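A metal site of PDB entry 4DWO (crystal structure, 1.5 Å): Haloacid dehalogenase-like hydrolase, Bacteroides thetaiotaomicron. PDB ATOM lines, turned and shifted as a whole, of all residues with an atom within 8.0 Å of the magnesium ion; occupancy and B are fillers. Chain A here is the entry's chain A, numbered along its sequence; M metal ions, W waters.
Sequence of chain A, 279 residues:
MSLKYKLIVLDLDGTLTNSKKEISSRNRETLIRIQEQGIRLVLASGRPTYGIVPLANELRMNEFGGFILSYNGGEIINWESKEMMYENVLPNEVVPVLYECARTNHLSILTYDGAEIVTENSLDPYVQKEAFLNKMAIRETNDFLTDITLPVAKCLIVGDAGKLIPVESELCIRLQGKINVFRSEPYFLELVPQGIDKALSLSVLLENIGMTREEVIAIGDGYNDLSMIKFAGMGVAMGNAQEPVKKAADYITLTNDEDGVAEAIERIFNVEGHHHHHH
Residues that only touch the magnesium ion: Asp 225 (3.9 Å). Within 4 Å of the magnesium ion: Asp 11, Asp 13, Asp 221 and Asp 225. The nearest printed residue that does not touch the magnesium ion is Thr 15 (4.2 Å).
Water W1 lies within hydrogen-bond range of the side-chain carboxylate (OD2) of Asp 225, the side-chain amide oxygen (OD1) of Asn 224 and the backbone NH (N) of Gly 222.
The magnesium ion is bound by the side-chain carboxylate of Asp 11, the backbone carbonyl oxygen of Asp 13, the side-chain carboxylate of Asp 221, water W1, water W3 and water W2.
The side-chain carboxylate of Asp 11 lies close to the side-chain hydroxyl of Thr 15 (3.1 Å). The side-chain carboxylate (OD1) of Asp 11 is in salt-bridge range of the side-chain amino group (NZ) of Lys 198, 2.8 Å away. The backbone carbonyl oxygen (O) of Asp 11 is in hydrogen-bond range of the backbone NH (N) of Leu 16, 3.2 Å away. The backbone NH (N) of Asp 11 sits at hydrogen-bond distance from the backbone carbonyl oxygen (O) of Ile 219. OD1 of Asp 13 is in salt-bridge range of NZ of Lys 21 (3.1 Å). The backbone NH (N) of Asp 221 is in hydrogen-bond range of the side-chain carboxylate (OD2) of Asp 225 (2.9 Å). N of Asp 221 is in hydrogen-bond range of OG1 of Thr 15 (3.4 Å). The backbone NH (N) of Gly 222 sits at hydrogen-bond distance from the side-chain carboxylate (OD2) of Asp 225, 3.3 Å away.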
ATOM      1  N   LEU A  10      20.663 -22.160  -9.161  1.00  0.00           N
ATOM      2  CA  LEU A  10      21.510 -21.370  -8.299  1.00  0.00           C
ATOM      3  C   LEU A  10      22.488 -20.498  -9.071  1.00  0.00           C
ATOM      4  O   LEU A  10      23.220 -21.007  -9.914  1.00  0.00           O
ATOM      5  CB  LEU A  10      22.353 -22.290  -7.421  1.00  0.00           C
ATOM      6  CG  LEU A  10      21.603 -23.335  -6.606  1.00  0.00           C
ATOM      7  CD1 LEU A  10      22.638 -24.224  -5.880  1.00  0.00           C
ATOM      8  CD2 LEU A  10      20.714 -22.642  -5.546  1.00  0.00           C
ATOM      9  N   ASP A  11      22.560 -19.214  -8.732  1.00  0.00           N
ATOM     10  CA  ASP A  11      23.709 -18.366  -9.082  1.00  0.00           C
ATOM     11  C   ASP A  11      24.940 -18.935  -8.289  1.00  0.00           C
ATOM     12  O   ASP A  11      24.769 -19.648  -7.291  1.00  0.00           O
ATOM     13  CB  ASP A  11      23.394 -16.911  -8.747  1.00  0.00           C
ATOM     14  CG  ASP A  11      24.554 -16.025  -8.934  1.00  0.00           C
ATOM     15  OD1 ASP A  11      25.136 -16.091 -10.038  1.00  0.00           O
ATOM     16  OD2 ASP A  11      24.878 -15.270  -7.967  1.00  0.00           O
ATOM     17  N   LEU A  12      26.144 -18.618  -8.773  1.00  0.00           N
ATOM     18  CA  LEU A  12      27.397 -19.008  -8.111  1.00  0.00           C
ATOM     19  C   LEU A  12      27.939 -17.943  -7.205  1.00  0.00           C
ATOM     20  O   LEU A  12      27.820 -18.089  -5.992  1.00  0.00           O
ATOM     21  CB  LEU A  12      28.435 -19.441  -9.133  1.00  0.00           C
ATOM     22  CG  LEU A  12      27.871 -20.605  -9.977  1.00  0.00           C
ATOM     23  CD1 LEU A  12      28.927 -21.034 -11.007  1.00  0.00           C
ATOM     24  CD2 LEU A  12      27.423 -21.801  -9.165  1.00  0.00           C
ATOM     25  N   ASP A  13      28.492 -16.881  -7.736  1.00  0.00           N
ATOM     26  CA  ASP A  13      29.219 -15.895  -6.944  1.00  0.00           C
ATOM     27  C   ASP A  13      28.233 -15.120  -6.118  1.00  0.00           C
ATOM     28  O   ASP A  13      27.241 -14.599  -6.644  1.00  0.00           O
ATOM     29  CB  ASP A  13      30.028 -14.964  -7.870  1.00  0.00           C
ATOM     30  CG  ASP A  13      31.106 -15.745  -8.641  1.00  0.00           C
ATOM     31  OD1 ASP A  13      32.132 -16.095  -8.049  1.00  0.00           O
ATOM     32  OD2 ASP A  13      30.941 -16.014  -9.857  1.00  0.00           O
ATOM     33  N   GLY A  14      28.444 -15.114  -4.803  1.00  0.00           N
ATOM     34  CA  GLY A  14      27.563 -14.410  -3.896  1.00  0.00           C
ATOM     35  C   GLY A  14      26.346 -15.222  -3.485  1.00  0.00           C
ATOM     36  O   GLY A  14      25.464 -14.696  -2.723  1.00  0.00           O
ATOM     37  N   THR A  15      26.208 -16.421  -4.038  1.00  0.00           N
ATOM     38  CA  THR A  15      25.018 -17.244  -3.769  1.00  0.00           C
ATOM     39  C   THR A  15      25.422 -18.634  -3.309  1.00  0.00           C
ATOM     40  O   THR A  15      25.481 -18.902  -2.094  1.00  0.00           O
ATOM     41  CB  THR A  15      24.100 -17.271  -5.035  1.00  0.00           C
ATOM     42  OG1 THR A  15      23.607 -15.943  -5.272  1.00  0.00           O
ATOM     43  CG2 THR A  15      22.888 -18.165  -4.769  1.00  0.00           C
ATOM     44  N   LEU A  16      25.787 -19.534  -4.232  1.00  0.00           N
ATOM     45  CA  LEU A  16      26.229 -20.870  -3.816  1.00  0.00           C
ATOM     46  C   LEU A  16      27.607 -20.830  -3.127  1.00  0.00           C
ATOM     47  O   LEU A  16      27.778 -21.495  -2.088  1.00  0.00           O
ATOM     48  CB  LEU A  16      26.304 -21.790  -5.022  1.00  0.00           C
ATOM     49  CG  LEU A  16      26.973 -23.132  -4.771  1.00  0.00           C
ATOM     50  CD1 LEU A  16      26.139 -23.962  -3.834  1.00  0.00           C
ATOM     51  CD2 LEU A  16      27.134 -23.826  -6.116  1.00  0.00           C
ATOM     52  N   THR A  17      28.550 -20.051  -3.643  1.00  0.00           N
ATOM     53  CA  THR A  17      29.871 -20.045  -3.044  1.00  0.00           C
ATOM     54  C   THR A  17      29.960 -18.980  -1.960  1.00  0.00           C
ATOM     55  O   THR A  17      29.258 -17.949  -1.987  1.00  0.00           O
ATOM     56  CB  THR A  17      30.970 -19.823  -4.095  1.00  0.00           C
ATOM     57  OG1 THR A  17      30.741 -18.595  -4.796  1.00  0.00           O
ATOM     58  CG2 THR A  17      30.933 -20.985  -5.102  1.00  0.00           C
ATOM     59  N   LYS A  21      35.003 -18.252  -2.235  1.00  0.00           N
ATOM     60  CA  LYS A  21      34.602 -18.833  -3.529  1.00  0.00           C
ATOM     61  C   LYS A  21      34.587 -20.355  -3.512  1.00  0.00           C
ATOM     62  O   LYS A  21      34.723 -21.002  -4.548  1.00  0.00           O
ATOM     63  CB  LYS A  21      35.486 -18.307  -4.669  1.00  0.00           C
ATOM     64  CG  LYS A  21      35.537 -16.756  -4.743  1.00  0.00           C
ATOM     65  CD  LYS A  21      34.248 -16.280  -5.406  1.00  0.00           C
ATOM     66  CE  LYS A  21      34.186 -14.774  -5.600  1.00  0.00           C
ATOM     67  NZ  LYS A  21      32.745 -14.354  -5.581  1.00  0.00           N
ATOM     68  N   ALA A  44      23.654 -21.452 -12.733  1.00  0.00           N
ATOM     69  CA  ALA A  44      23.448 -20.412 -13.754  1.00  0.00           C
ATOM     70  C   ALA A  44      24.336 -19.271 -13.433  1.00  0.00           C
ATOM     71  O   ALA A  44      24.136 -18.612 -12.409  1.00  0.00           O
ATOM     72  CB  ALA A  44      22.003 -19.961 -13.732  1.00  0.00           C
ATOM     73  N   SER A  45      25.245 -18.916 -14.362  1.00  0.00           N
ATOM     74  CA  SER A  45      26.273 -17.943 -14.066  1.00  0.00           C
ATOM     75  C   SER A  45      26.755 -17.224 -15.334  1.00  0.00           C
ATOM     76  O   SER A  45      26.665 -17.835 -16.416  1.00  0.00           O
ATOM     77  CB  SER A  45      27.441 -18.759 -13.460  1.00  0.00           C
ATOM     78  OG  SER A  45      28.562 -17.947 -13.194  1.00  0.00           O
ATOM     79  N   GLY A  46      27.347 -16.047 -15.165  1.00  0.00           N
ATOM     80  CA  GLY A  46      28.063 -15.375 -16.253  1.00  0.00           C
ATOM     81  C   GLY A  46      29.358 -16.090 -16.637  1.00  0.00           C
ATOM     82  O   GLY A  46      29.896 -15.932 -17.727  1.00  0.00           O
ATOM     83  N   GLU A 185      30.553  -7.695 -12.211  1.00  0.00           N
ATOM     84  CA  GLU A 185      31.326  -6.938 -11.208  1.00  0.00           C
ATOM     85  C   GLU A 185      31.542  -5.539 -11.814  1.00  0.00           C
ATOM     86  O   GLU A 185      31.456  -5.374 -13.031  1.00  0.00           O
ATOM     87  CB  GLU A 185      32.703  -7.566 -10.980  1.00  0.00           C
ATOM     88  CG  GLU A 185      32.670  -8.983 -10.441  1.00  0.00           C
ATOM     89  CD  GLU A 185      32.022  -9.070  -9.073  1.00  0.00           C
ATOM     90  OE1 GLU A 185      31.608 -10.191  -8.701  1.00  0.00           O
ATOM     91  OE2 GLU A 185      31.936  -8.019  -8.385  1.00  0.00           O
ATOM     92  N   LYS A 198      19.743 -14.863 -17.804  1.00  0.00           N
ATOM     93  CA  LYS A 198      19.435 -16.130 -17.103  1.00  0.00           C
ATOM     94  C   LYS A 198      17.980 -16.563 -17.200  1.00  0.00           C
ATOM     95  O   LYS A 198      17.678 -17.759 -17.275  1.00  0.00           O
ATOM     96  CB  LYS A 198      19.835 -16.092 -15.626  1.00  0.00           C
ATOM     97  CG  LYS A 198      21.375 -15.977 -15.439  1.00  0.00           C
ATOM     98  CD  LYS A 198      21.704 -15.939 -13.922  1.00  0.00           C
ATOM     99  CE  LYS A 198      23.133 -15.488 -13.753  1.00  0.00           C
ATOM    100  NZ  LYS A 198      23.552 -15.561 -12.326  1.00  0.00           N
ATOM    101  N   ILE A 219      17.591 -19.033  -6.948  1.00  0.00           N
ATOM    102  CA  ILE A 219      18.234 -18.329  -5.833  1.00  0.00           C
ATOM    103  C   ILE A 219      19.369 -17.504  -6.372  1.00  0.00           C
ATOM    104  O   ILE A 219      20.223 -18.000  -7.111  1.00  0.00           O
ATOM    105  CB  ILE A 219      18.793 -19.336  -4.805  1.00  0.00           C
ATOM    106  CG1 ILE A 219      17.749 -20.411  -4.458  1.00  0.00           C
ATOM    107  CG2 ILE A 219      19.308 -18.588  -3.564  1.00  0.00           C
ATOM    108  CD1 ILE A 219      18.124 -21.268  -3.237  1.00  0.00           C
ATOM    109  N   GLY A 220      19.417 -16.221  -6.013  1.00  0.00           N
ATOM    110  CA  GLY A 220      20.538 -15.378  -6.451  1.00  0.00           C
ATOM    111  C   GLY A 220      20.675 -14.134  -5.587  1.00  0.00           C
ATOM    112  O   GLY A 220      19.994 -13.942  -4.607  1.00  0.00           O
ATOM    113  N   ASP A 221      21.588 -13.265  -5.986  1.00  0.00           N
ATOM    114  CA  ASP A 221      21.965 -12.131  -5.148  1.00  0.00           C
ATOM    115  C   ASP A 221      22.018 -10.789  -5.918  1.00  0.00           C
ATOM    116  O   ASP A 221      21.566  -9.712  -5.443  1.00  0.00           O
ATOM    117  CB  ASP A 221      23.279 -12.375  -4.367  1.00  0.00           C
ATOM    118  CG  ASP A 221      24.510 -12.420  -5.251  1.00  0.00           C
ATOM    119  OD1 ASP A 221      24.592 -13.214  -6.220  1.00  0.00           O
ATOM    120  OD2 ASP A 221      25.470 -11.612  -4.999  1.00  0.00           O
ATOM    121  N   GLY A 222      22.514 -10.861  -7.143  1.00  0.00           N
ATOM    122  CA  GLY A 222      22.871  -9.692  -7.922  1.00  0.00           C
ATOM    123  C   GLY A 222      21.748  -9.219  -8.806  1.00  0.00           C
ATOM    124  O   GLY A 222      20.789  -9.952  -9.004  1.00  0.00           O
ATOM    125  N   TYR A 223      21.852  -7.992  -9.335  1.00  0.00           N
ATOM    126  CA  TYR A 223      20.869  -7.514 -10.276  1.00  0.00           C
ATOM    127  C   TYR A 223      20.754  -8.416 -11.503  1.00  0.00           C
ATOM    128  O   TYR A 223      19.680  -8.543 -12.093  1.00  0.00           O
ATOM    129  CB  TYR A 223      21.176  -6.076 -10.717  1.00  0.00           C
ATOM    130  CG  TYR A 223      20.835  -4.997  -9.670  1.00  0.00           C
ATOM    131  CD1 TYR A 223      19.545  -4.871  -9.180  1.00  0.00           C
ATOM    132  CD2 TYR A 223      21.811  -4.183  -9.157  1.00  0.00           C
ATOM    133  CE1 TYR A 223      19.234  -3.865  -8.222  1.00  0.00           C
ATOM    134  CE2 TYR A 223      21.512  -3.207  -8.205  1.00  0.00           C
ATOM    135  CZ  TYR A 223      20.225  -3.090  -7.714  1.00  0.00           C
ATOM    136  OH  TYR A 223      19.969  -2.097  -6.785  1.00  0.00           O
ATOM    137  N   ASN A 224      21.835  -9.098 -11.858  1.00  0.00           N
ATOM    138  CA  ASN A 224      21.745 -10.055 -12.976  1.00  0.00           C
ATOM    139  C   ASN A 224      20.923 -11.288 -12.666  1.00  0.00           C
ATOM    140  O   ASN A 224      20.653 -12.098 -13.558  1.00  0.00           O
ATOM    141  CB  ASN A 224      23.153 -10.471 -13.487  1.00  0.00           C
ATOM    142  CG  ASN A 224      23.958 -11.261 -12.445  1.00  0.00           C
ATOM    143  OD1 ASN A 224      23.641 -11.262 -11.245  1.00  0.00           O
ATOM    144  ND2 ASN A 224      25.033 -11.924 -12.904  1.00  0.00           N
ATOM    145  N   ASP A 225      20.520 -11.470 -11.408  1.00  0.00           N
ATOM    146  CA  ASP A 225      19.618 -12.544 -11.040  1.00  0.00           C
ATOM    147  C   ASP A 225      18.157 -12.106 -10.861  1.00  0.00           C
ATOM    148  O   ASP A 225      17.302 -12.946 -10.596  1.00  0.00           O
ATOM    149  CB  ASP A 225      20.041 -13.172  -9.697  1.00  0.00           C
ATOM    150  CG  ASP A 225      21.398 -13.799  -9.786  1.00  0.00           C
ATOM    151  OD1 ASP A 225      21.739 -14.411 -10.824  1.00  0.00           O
ATOM    152  OD2 ASP A 225      22.195 -13.678  -8.827  1.00  0.00           O
ATOM    153  N   MET A 228      15.512 -13.896 -13.176  1.00  0.00           N
ATOM    154  CA  MET A 228      15.209 -15.267 -12.926  1.00  0.00           C
ATOM    155  C   MET A 228      14.483 -15.453 -11.573  1.00  0.00           C
ATOM    156  O   MET A 228      13.684 -16.344 -11.426  1.00  0.00           O
ATOM    157  CB  MET A 228      16.415 -16.217 -13.055  1.00  0.00           C
ATOM    158  CG  MET A 228      17.393 -16.187 -11.903  1.00  0.00           C
ATOM    159  SD  MET A 228      18.563 -17.592 -12.042  1.00  0.00           S
ATOM    160  CE  MET A 228      19.560 -17.226 -10.567  1.00  0.00           C
ATOM    161  N   MET A 238      19.378 -13.939  -1.746  1.00  0.00           N
ATOM    162  CA  MET A 238      20.356 -14.122  -0.650  1.00  0.00           C
ATOM    163  C   MET A 238      20.318 -12.952   0.339  1.00  0.00           C
ATOM    164  O   MET A 238      19.897 -11.823   0.013  1.00  0.00           O
ATOM    165  CB  MET A 238      21.761 -14.234  -1.223  1.00  0.00           C
ATOM    166  CG  MET A 238      21.929 -15.438  -2.185  1.00  0.00           C
ATOM    167  SD  MET A 238      21.641 -17.028  -1.390  1.00  0.00           S
ATOM    168  CE  MET A 238      23.025 -17.095  -0.211  1.00  0.00           C
ATOM    169  N   ASN A 240      22.647 -11.236   1.301  1.00  0.00           N
ATOM    170  CA  ASN A 240      23.578 -10.235   0.798  1.00  0.00           C
ATOM    171  C   ASN A 240      23.124  -9.661  -0.561  1.00  0.00           C
ATOM    172  O   ASN A 240      23.865  -8.895  -1.184  1.00  0.00           O
ATOM    173  CB  ASN A 240      24.984 -10.839   0.704  1.00  0.00           C
ATOM    174  CG  ASN A 240      24.991 -12.184  -0.027  1.00  0.00           C
ATOM    175  OD1 ASN A 240      24.564 -13.190   0.560  1.00  0.00           O
ATOM    176  ND2 ASN A 240      25.502 -12.210  -1.250  1.00  0.00           N
ATOM    177  N   ASN A 256      25.441 -15.732   1.724  1.00  0.00           N
ATOM    178  CA  ASN A 256      26.189 -16.857   1.147  1.00  0.00           C
ATOM    179  C   ASN A 256      27.092 -17.497   2.171  1.00  0.00           C
ATOM    180  O   ASN A 256      27.105 -18.721   2.317  1.00  0.00           O
ATOM    181  CB  ASN A 256      26.914 -16.494  -0.115  1.00  0.00           C
ATOM    182  CG  ASN A 256      27.888 -15.340   0.056  1.00  0.00           C
ATOM    183  OD1 ASN A 256      27.665 -14.394   0.819  1.00  0.00           O
ATOM    184  ND2 ASN A 256      28.969 -15.416  -0.681  1.00  0.00           N
HETATM  185 MG    MG M   1      25.904 -13.532  -7.799  1.00  0.00          MG
HETATM  186  O   HOH W   1      24.549 -12.531  -9.095  1.00  0.00           O
HETATM  187  O   HOH W   2      26.881 -11.680  -7.324  1.00  0.00           O
HETATM  188  O   HOH W   3      27.088 -13.855  -9.541  1.00  0.00           O
